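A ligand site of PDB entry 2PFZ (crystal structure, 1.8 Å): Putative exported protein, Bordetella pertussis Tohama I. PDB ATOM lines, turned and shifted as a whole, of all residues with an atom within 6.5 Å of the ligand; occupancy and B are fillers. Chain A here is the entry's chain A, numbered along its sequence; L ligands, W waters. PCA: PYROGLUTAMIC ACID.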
ATOM      1  N   TYR A   9     -18.295  27.666 -24.612  1.00  0.00           N
ATOM      2  CA  TYR A   9     -19.011  27.842 -25.886  1.00  0.00           C
ATOM      3  C   TYR A   9     -18.067  28.266 -27.005  1.00  0.00           C
ATOM      4  O   TYR A   9     -16.968  28.775 -26.713  1.00  0.00           O
ATOM      5  CB  TYR A   9     -20.167  28.849 -25.676  1.00  0.00           C
ATOM      6  CG  TYR A   9     -20.954  28.450 -24.469  1.00  0.00           C
ATOM      7  CD1 TYR A   9     -21.796  27.342 -24.512  1.00  0.00           C
ATOM      8  CD2 TYR A   9     -20.815  29.118 -23.260  1.00  0.00           C
ATOM      9  CE1 TYR A   9     -22.479  26.937 -23.411  1.00  0.00           C
ATOM     10  CE2 TYR A   9     -21.485  28.716 -22.154  1.00  0.00           C
ATOM     11  CZ  TYR A   9     -22.347  27.618 -22.236  1.00  0.00           C
ATOM     12  OH  TYR A   9     -23.020  27.186 -21.121  1.00  0.00           O
ATOM     13  N   ASN A  13     -20.543  31.632 -30.937  1.00  0.00           N
ATOM     14  CA  ASN A  13     -21.607  31.862 -29.965  1.00  0.00           C
ATOM     15  C   ASN A  13     -21.674  33.311 -29.476  1.00  0.00           C
ATOM     16  O   ASN A  13     -20.637  33.966 -29.226  1.00  0.00           O
ATOM     17  CB  ASN A  13     -21.477  30.841 -28.836  1.00  0.00           C
ATOM     18  CG  ASN A  13     -22.397  31.144 -27.656  1.00  0.00           C
ATOM     19  OD1 ASN A  13     -23.548  30.681 -27.602  1.00  0.00           O
ATOM     20  ND2 ASN A  13     -21.888  31.923 -26.736  1.00  0.00           N
ATOM     21  N   LEU A  65     -22.455  29.083 -16.556  1.00  0.00           N
ATOM     22  CA  LEU A  65     -23.912  29.105 -16.696  1.00  0.00           C
ATOM     23  C   LEU A  65     -24.419  28.940 -15.287  1.00  0.00           C
ATOM     24  O   LEU A  65     -24.137  27.912 -14.653  1.00  0.00           O
ATOM     25  CB  LEU A  65     -24.383  27.896 -17.512  1.00  0.00           C
ATOM     26  CG  LEU A  65     -25.895  27.713 -17.630  1.00  0.00           C
ATOM     27  CD1 LEU A  65     -26.440  28.756 -18.550  1.00  0.00           C
ATOM     28  CD2 LEU A  65     -26.203  26.273 -18.098  1.00  0.00           C
ATOM     29  N   TRP A 119     -29.088  34.188 -21.944  1.00  0.00           N
ATOM     30  CA  TRP A 119     -29.306  33.457 -23.189  1.00  0.00           C
ATOM     31  C   TRP A 119     -30.730  33.802 -23.671  1.00  0.00           C
ATOM     32  O   TRP A 119     -31.557  34.267 -22.886  1.00  0.00           O
ATOM     33  CB  TRP A 119     -29.266  31.938 -22.916  1.00  0.00           C
ATOM     34  CG  TRP A 119     -27.893  31.340 -22.721  1.00  0.00           C
ATOM     35  CD1 TRP A 119     -27.203  31.215 -21.550  1.00  0.00           C
ATOM     36  CD2 TRP A 119     -27.095  30.730 -23.727  1.00  0.00           C
ATOM     37  NE1 TRP A 119     -26.009  30.567 -21.757  1.00  0.00           N
ATOM     38  CE2 TRP A 119     -25.910  30.267 -23.099  1.00  0.00           C
ATOM     39  CE3 TRP A 119     -27.244  30.550 -25.104  1.00  0.00           C
ATOM     40  CZ2 TRP A 119     -24.902  29.615 -23.797  1.00  0.00           C
ATOM     41  CZ3 TRP A 119     -26.239  29.908 -25.804  1.00  0.00           C
ATOM     42  CH2 TRP A 119     -25.084  29.443 -25.148  1.00  0.00           C
ATOM     43  N   PRO A 120     -31.014  33.575 -24.970  1.00  0.00           N
ATOM     44  CA  PRO A 120     -32.383  33.803 -25.482  1.00  0.00           C
ATOM     45  C   PRO A 120     -33.457  32.868 -24.864  1.00  0.00           C
ATOM     46  O   PRO A 120     -33.134  31.862 -24.210  1.00  0.00           O
ATOM     47  CB  PRO A 120     -32.225  33.583 -26.976  1.00  0.00           C
ATOM     48  CG  PRO A 120     -30.688  33.856 -27.225  1.00  0.00           C
ATOM     49  CD  PRO A 120     -30.093  33.205 -26.054  1.00  0.00           C
ATOM     50  N   GLN A 122     -36.026  30.118 -23.877  1.00  0.00           N
ATOM     51  CA  GLN A 122     -35.805  28.700 -24.106  1.00  0.00           C
ATOM     52  C   GLN A 122     -37.002  27.993 -24.676  1.00  0.00           C
ATOM     53  O   GLN A 122     -38.090  28.062 -24.094  1.00  0.00           O
ATOM     54  CB  GLN A 122     -35.397  28.009 -22.822  1.00  0.00           C
ATOM     55  CG  GLN A 122     -34.187  28.703 -22.165  1.00  0.00           C
ATOM     56  CD  GLN A 122     -32.841  28.351 -22.774  1.00  0.00           C
ATOM     57  OE1 GLN A 122     -32.173  29.194 -23.388  1.00  0.00           O
ATOM     58  NE2 GLN A 122     -32.417  27.139 -22.563  1.00  0.00           N
ATOM     59  N   ARG A 142     -31.972  15.787 -23.932  1.00  0.00           N
ATOM     60  CA  ARG A 142     -30.657  16.289 -23.573  1.00  0.00           C
ATOM     61  C   ARG A 142     -30.789  17.428 -22.560  1.00  0.00           C
ATOM     62  O   ARG A 142     -31.379  18.481 -22.844  1.00  0.00           O
ATOM     63  CB  ARG A 142     -29.909  16.745 -24.822  1.00  0.00           C
ATOM     64  CG  ARG A 142     -28.551  17.458 -24.550  1.00  0.00           C
ATOM     65  CD  ARG A 142     -28.701  19.005 -24.571  1.00  0.00           C
ATOM     66  NE  ARG A 142     -27.457  19.719 -24.278  1.00  0.00           N
ATOM     67  CZ  ARG A 142     -27.309  21.040 -24.409  1.00  0.00           C
ATOM     68  NH1 ARG A 142     -28.331  21.794 -24.851  1.00  0.00           N
ATOM     69  NH2 ARG A 142     -26.138  21.597 -24.097  1.00  0.00           N
ATOM     70  N   TYR A 144     -28.858  20.242 -20.110  1.00  0.00           N
ATOM     71  CA  TYR A 144     -27.616  20.993 -20.031  1.00  0.00           C
ATOM     72  C   TYR A 144     -27.362  21.472 -18.601  1.00  0.00           C
ATOM     73  O   TYR A 144     -26.384  22.171 -18.323  1.00  0.00           O
ATOM     74  CB  TYR A 144     -27.636  22.158 -21.045  1.00  0.00           C
ATOM     75  CG  TYR A 144     -28.681  23.252 -20.821  1.00  0.00           C
ATOM     76  CD1 TYR A 144     -29.741  23.430 -21.711  1.00  0.00           C
ATOM     77  CD2 TYR A 144     -28.607  24.100 -19.696  1.00  0.00           C
ATOM     78  CE1 TYR A 144     -30.697  24.436 -21.508  1.00  0.00           C
ATOM     79  CE2 TYR A 144     -29.549  25.109 -19.489  1.00  0.00           C
ATOM     80  CZ  TYR A 144     -30.602  25.273 -20.412  1.00  0.00           C
ATOM     81  OH  TYR A 144     -31.538  26.268 -20.238  1.00  0.00           O
ATOM     82  N   VAL A 162     -25.596  16.557 -21.573  1.00  0.00           N
ATOM     83  CA  VAL A 162     -24.600  16.705 -22.611  1.00  0.00           C
ATOM     84  C   VAL A 162     -24.230  18.169 -22.716  1.00  0.00           C
ATOM     85  O   VAL A 162     -25.099  19.025 -22.973  1.00  0.00           O
ATOM     86  CB  VAL A 162     -25.109  16.203 -23.992  1.00  0.00           C
ATOM     87  CG1 VAL A 162     -23.972  16.151 -24.978  1.00  0.00           C
ATOM     88  CG2 VAL A 162     -25.755  14.841 -23.870  1.00  0.00           C
ATOM     89  N   GLN A 163     -22.939  18.481 -22.536  1.00  0.00           N
ATOM     90  CA  GLN A 163     -22.501  19.877 -22.702  1.00  0.00           C
ATOM     91  C   GLN A 163     -22.645  20.306 -24.148  1.00  0.00           C
ATOM     92  O   GLN A 163     -22.682  19.453 -25.028  1.00  0.00           O
ATOM     93  CB  GLN A 163     -21.087  20.084 -22.177  1.00  0.00           C
ATOM     94  CG  GLN A 163     -20.956  19.633 -20.717  1.00  0.00           C
ATOM     95  CD  GLN A 163     -21.952  20.342 -19.811  1.00  0.00           C
ATOM     96  OE1 GLN A 163     -22.282  21.508 -20.046  1.00  0.00           O
ATOM     97  NE2 GLN A 163     -22.474  19.642 -18.815  1.00  0.00           N
ATOM     98  N   GLN A 164     -22.716  21.615 -24.398  1.00  0.00           N
ATOM     99  CA  GLN A 164     -22.920  22.095 -25.772  1.00  0.00           C
ATOM    100  C   GLN A 164     -21.796  21.636 -26.703  1.00  0.00           C
ATOM    101  O   GLN A 164     -22.037  21.347 -27.870  1.00  0.00           O
ATOM    102  CB  GLN A 164     -23.063  23.620 -25.872  1.00  0.00           C
ATOM    103  CG  GLN A 164     -23.508  24.049 -27.264  1.00  0.00           C
ATOM    104  CD  GLN A 164     -23.881  25.532 -27.400  1.00  0.00           C
ATOM    105  OE1 GLN A 164     -23.494  26.200 -28.357  1.00  0.00           O
ATOM    106  NE2 GLN A 164     -24.642  26.024 -26.461  1.00  0.00           N
ATOM    107  N   LEU A 167     -22.770  18.319 -28.037  1.00  0.00           N
ATOM    108  CA  LEU A 167     -24.181  18.153 -28.437  1.00  0.00           C
ATOM    109  C   LEU A 167     -24.320  17.645 -29.871  1.00  0.00           C
ATOM    110  O   LEU A 167     -25.120  16.765 -30.154  1.00  0.00           O
ATOM    111  CB  LEU A 167     -24.917  19.489 -28.324  1.00  0.00           C
ATOM    112  CG  LEU A 167     -26.358  19.557 -27.811  1.00  0.00           C
ATOM    113  CD1 LEU A 167     -26.984  20.896 -28.141  1.00  0.00           C
ATOM    114  CD2 LEU A 167     -27.258  18.413 -28.194  1.00  0.00           C
ATOM    115  N   TYR A 179     -34.520  18.401 -26.800  1.00  0.00           N
ATOM    116  CA  TYR A 179     -34.005  19.191 -25.691  1.00  0.00           C
ATOM    117  C   TYR A 179     -34.615  20.600 -25.602  1.00  0.00           C
ATOM    118  O   TYR A 179     -35.192  21.093 -26.557  1.00  0.00           O
ATOM    119  CB  TYR A 179     -32.475  19.271 -25.715  1.00  0.00           C
ATOM    120  CG  TYR A 179     -31.829  20.061 -26.819  1.00  0.00           C
ATOM    121  CD1 TYR A 179     -31.646  19.491 -28.085  1.00  0.00           C
ATOM    122  CD2 TYR A 179     -31.325  21.346 -26.600  1.00  0.00           C
ATOM    123  CE1 TYR A 179     -31.028  20.205 -29.109  1.00  0.00           C
ATOM    124  CE2 TYR A 179     -30.726  22.068 -27.617  1.00  0.00           C
ATOM    125  CZ  TYR A 179     -30.573  21.483 -28.876  1.00  0.00           C
ATOM    126  OH  TYR A 179     -29.933  22.180 -29.906  1.00  0.00           O
ATOM    127  N   MET A 180     -34.467  21.241 -24.447  1.00  0.00           N
ATOM    128  CA  MET A 180     -34.748  22.676 -24.353  1.00  0.00           C
ATOM    129  C   MET A 180     -33.471  23.496 -24.344  1.00  0.00           C
ATOM    130  O   MET A 180     -32.487  23.105 -23.716  1.00  0.00           O
ATOM    131  CB  MET A 180     -35.643  23.014 -23.182  1.00  0.00           C
ATOM    132  CG  MET A 180     -37.065  22.468 -23.364  1.00  0.00           C
ATOM    133  SD  MET A 180     -38.183  22.910 -22.032  1.00  0.00           S
ATOM    134  CE  MET A 180     -38.519  24.619 -22.416  1.00  0.00           C
ATOM    135  N   SER A 181     -33.485  24.561 -25.152  1.00  0.00           N
ATOM    136  CA  SER A 181     -32.359  25.510 -25.296  1.00  0.00           C
ATOM    137  C   SER A 181     -32.842  26.679 -26.154  1.00  0.00           C
ATOM    138  O   SER A 181     -34.042  26.839 -26.400  1.00  0.00           O
ATOM    139  CB  SER A 181     -31.156  24.858 -25.987  1.00  0.00           C
ATOM    140  OG  SER A 181     -30.006  25.689 -25.873  1.00  0.00           O
ATOM    141  N   SER A 182     -31.884  27.503 -26.607  1.00  0.00           N
ATOM    142  CA  SER A 182     -32.150  28.711 -27.364  1.00  0.00           C
ATOM    143  C   SER A 182     -32.034  28.408 -28.873  1.00  0.00           C
ATOM    144  O   SER A 182     -31.485  27.384 -29.251  1.00  0.00           O
ATOM    145  CB  SER A 182     -31.148  29.783 -26.978  1.00  0.00           C
ATOM    146  OG  SER A 182     -29.817  29.297 -27.123  1.00  0.00           O
ATOM    147  N   GLY A 183     -32.571  29.301 -29.701  1.00  0.00           N
ATOM    148  CA  GLY A 183     -32.326  29.242 -31.142  1.00  0.00           C
ATOM    149  C   GLY A 183     -30.835  29.333 -31.435  1.00  0.00           C
ATOM    150  O   GLY A 183     -30.350  28.719 -32.391  1.00  0.00           O
ATOM    151  N   SER A 184     -30.129  30.144 -30.631  1.00  0.00           N
ATOM    152  CA  SER A 184     -28.666  30.282 -30.660  1.00  0.00           C
ATOM    153  C   SER A 184     -27.973  28.917 -30.710  1.00  0.00           C
ATOM    154  O   SER A 184     -27.302  28.594 -31.696  1.00  0.00           O
ATOM    155  CB  SER A 184     -28.188  31.082 -29.445  1.00  0.00           C
ATOM    156  OG  SER A 184     -26.775  31.015 -29.270  1.00  0.00           O
ATOM    157  N   THR A 185     -28.148  28.132 -29.655  1.00  0.00           N
ATOM    158  CA  THR A 185     -27.569  26.779 -29.550  1.00  0.00           C
ATOM    159  C   THR A 185     -28.042  25.853 -30.655  1.00  0.00           C
ATOM    160  O   THR A 185     -27.217  25.120 -31.243  1.00  0.00           O
ATOM    161  CB  THR A 185     -27.822  26.165 -28.170  1.00  0.00           C
ATOM    162  OG1 THR A 185     -27.118  26.930 -27.204  1.00  0.00           O
ATOM    163  CG2 THR A 185     -27.318  24.726 -28.120  1.00  0.00           C
ATOM    164  N   TRP A 204     -37.919  30.170 -20.089  1.00  0.00           N
ATOM    165  CA  TRP A 204     -37.044  30.871 -19.156  1.00  0.00           C
ATOM    166  C   TRP A 204     -35.905  31.467 -19.969  1.00  0.00           C
ATOM    167  O   TRP A 204     -35.789  31.184 -21.163  1.00  0.00           O
ATOM    168  CB  TRP A 204     -36.526  29.940 -18.023  1.00  0.00           C
ATOM    169  CG  TRP A 204     -35.573  28.860 -18.422  1.00  0.00           C
ATOM    170  CD1 TRP A 204     -34.191  28.927 -18.405  1.00  0.00           C
ATOM    171  CD2 TRP A 204     -35.908  27.553 -18.867  1.00  0.00           C
ATOM    172  NE1 TRP A 204     -33.649  27.734 -18.861  1.00  0.00           N
ATOM    173  CE2 TRP A 204     -34.690  26.867 -19.144  1.00  0.00           C
ATOM    174  CE3 TRP A 204     -37.124  26.886 -19.094  1.00  0.00           C
ATOM    175  CZ2 TRP A 204     -34.649  25.550 -19.609  1.00  0.00           C
ATOM    176  CZ3 TRP A 204     -37.094  25.556 -19.562  1.00  0.00           C
ATOM    177  CH2 TRP A 204     -35.860  24.908 -19.822  1.00  0.00           C
ATOM    178  N   PRO A 206     -31.956  31.584 -19.228  1.00  0.00           N
ATOM    179  CA  PRO A 206     -30.919  31.302 -18.254  1.00  0.00           C
ATOM    180  C   PRO A 206     -29.731  32.223 -18.525  1.00  0.00           C
ATOM    181  O   PRO A 206     -29.456  32.549 -19.669  1.00  0.00           O
ATOM    182  CB  PRO A 206     -30.542  29.848 -18.584  1.00  0.00           C
ATOM    183  CG  PRO A 206     -30.787  29.705 -20.050  1.00  0.00           C
ATOM    184  CD  PRO A 206     -31.885  30.716 -20.407  1.00  0.00           C
ATOM    185  N   ASN A 208     -25.574  33.330 -18.314  1.00  0.00           N
ATOM    186  CA  ASN A 208     -24.158  33.123 -17.990  1.00  0.00           C
ATOM    187  C   ASN A 208     -23.680  34.236 -17.074  1.00  0.00           C
ATOM    188  O   ASN A 208     -24.315  35.296 -17.006  1.00  0.00           O
ATOM    189  CB  ASN A 208     -23.323  33.075 -19.276  1.00  0.00           C
ATOM    190  CG  ASN A 208     -23.545  31.790 -20.044  1.00  0.00           C
ATOM    191  OD1 ASN A 208     -24.266  30.901 -19.586  1.00  0.00           O
ATOM    192  ND2 ASN A 208     -22.955  31.699 -21.221  1.00  0.00           N
HETATM  193  N   PCA L   1     -27.749  27.165 -24.696  1.00  0.00           N
HETATM  194  CA  PCA L   1     -26.881  26.547 -23.667  1.00  0.00           C
HETATM  195  CB  PCA L   1     -27.415  26.862 -22.265  1.00  0.00           C
HETATM  196  CG  PCA L   1     -28.680  27.667 -22.465  1.00  0.00           C
HETATM  197  CD  PCA L   1     -28.765  27.845 -23.943  1.00  0.00           C
HETATM  198  OE  PCA L   1     -29.622  28.564 -24.490  1.00  0.00           O
HETATM  199  C   PCA L   1     -26.963  25.052 -23.865  1.00  0.00           C
HETATM  200  O   PCA L   1     -26.121  24.289 -23.379  1.00  0.00           O
HETATM  201  OXT PCA L   1     -27.906  24.596 -24.543  1.00  0.00           O
HETATM  202  O   HOH W   1     -24.329  24.920 -21.481  1.00  0.00           O
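OE1 of Gln 122 sits close to O of Pro 120, 3.0 Å away.
The side-chain amide nitrogen of Gln 122 is in hydrogen-bond range of the side-chain hydroxyl of Tyr 144, at 2.6 Å.
The backbone NH of Trp 119 is in hydrogen-bond range of the backbone carbonyl oxygen of Pro 206, 2.8 Å away.
The side-chain amide oxygen (OD1) of Asn 208 sits at hydrogen-bond distance from the indole nitrogen (NE1) of Trp 119 (2.8 Å).
OG1 of Thr 185 sits at hydrogen-bond distance from NE2 of Gln 164, 2.7 Å away.
N of Gln 122 is in hydrogen-bond range of O of Trp 204 (2.9 Å).
The side-chain hydroxyl of Tyr 144 is in hydrogen-bond range of the indole nitrogen of Trp 204, at 2.9 Å.
OG1 of Thr 185 lies close to OG of Ser 181, at 3.4 Å.
Residues that only touch the ligand: Trp 119 (3.2 Å), Tyr 144 (3.5 Å), Gln 164 (3.6 Å) and Pro 206 (3.8 Å).
Hydrophobic or aromatic side chains that line the ligand: Trp 119, Tyr 144 and Pro 206.
Within 4 Å of the ligand: Trp 119, Gln 122, Arg 142, Tyr 144, Gln 164, Ser 181, Ser 182, Thr 185 and Pro 206.
The nearest printed residue that does not touch the ligand is Leu 65 (4.3 Å).
N of Ser 182 sits close to OE of the ligand (3.3 Å).
OG of Ser 182 is in hydrogen-bond range of OE of the ligand (2.7 Å).
The side-chain hydroxyl of Ser 181 is in hydrogen-bond range of an oxygen (OXT) of the ligand, at 2.7 Å.
A nitrogen (N) of the ligand is in hydrogen-bond range of the side-chain hydroxyl (OG1) of Thr 185 (2.6 Å).
An oxygen (OE) of the ligand sits close to the side-chain amide oxygen (OE1) of Gln 122.
NH2 of Arg 142 is in salt-bridge range of O of the ligand.
Water W1 lies within hydrogen-bond range of OH of Tyr 9 (2.6 Å) and O of the ligand (2.7 Å).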
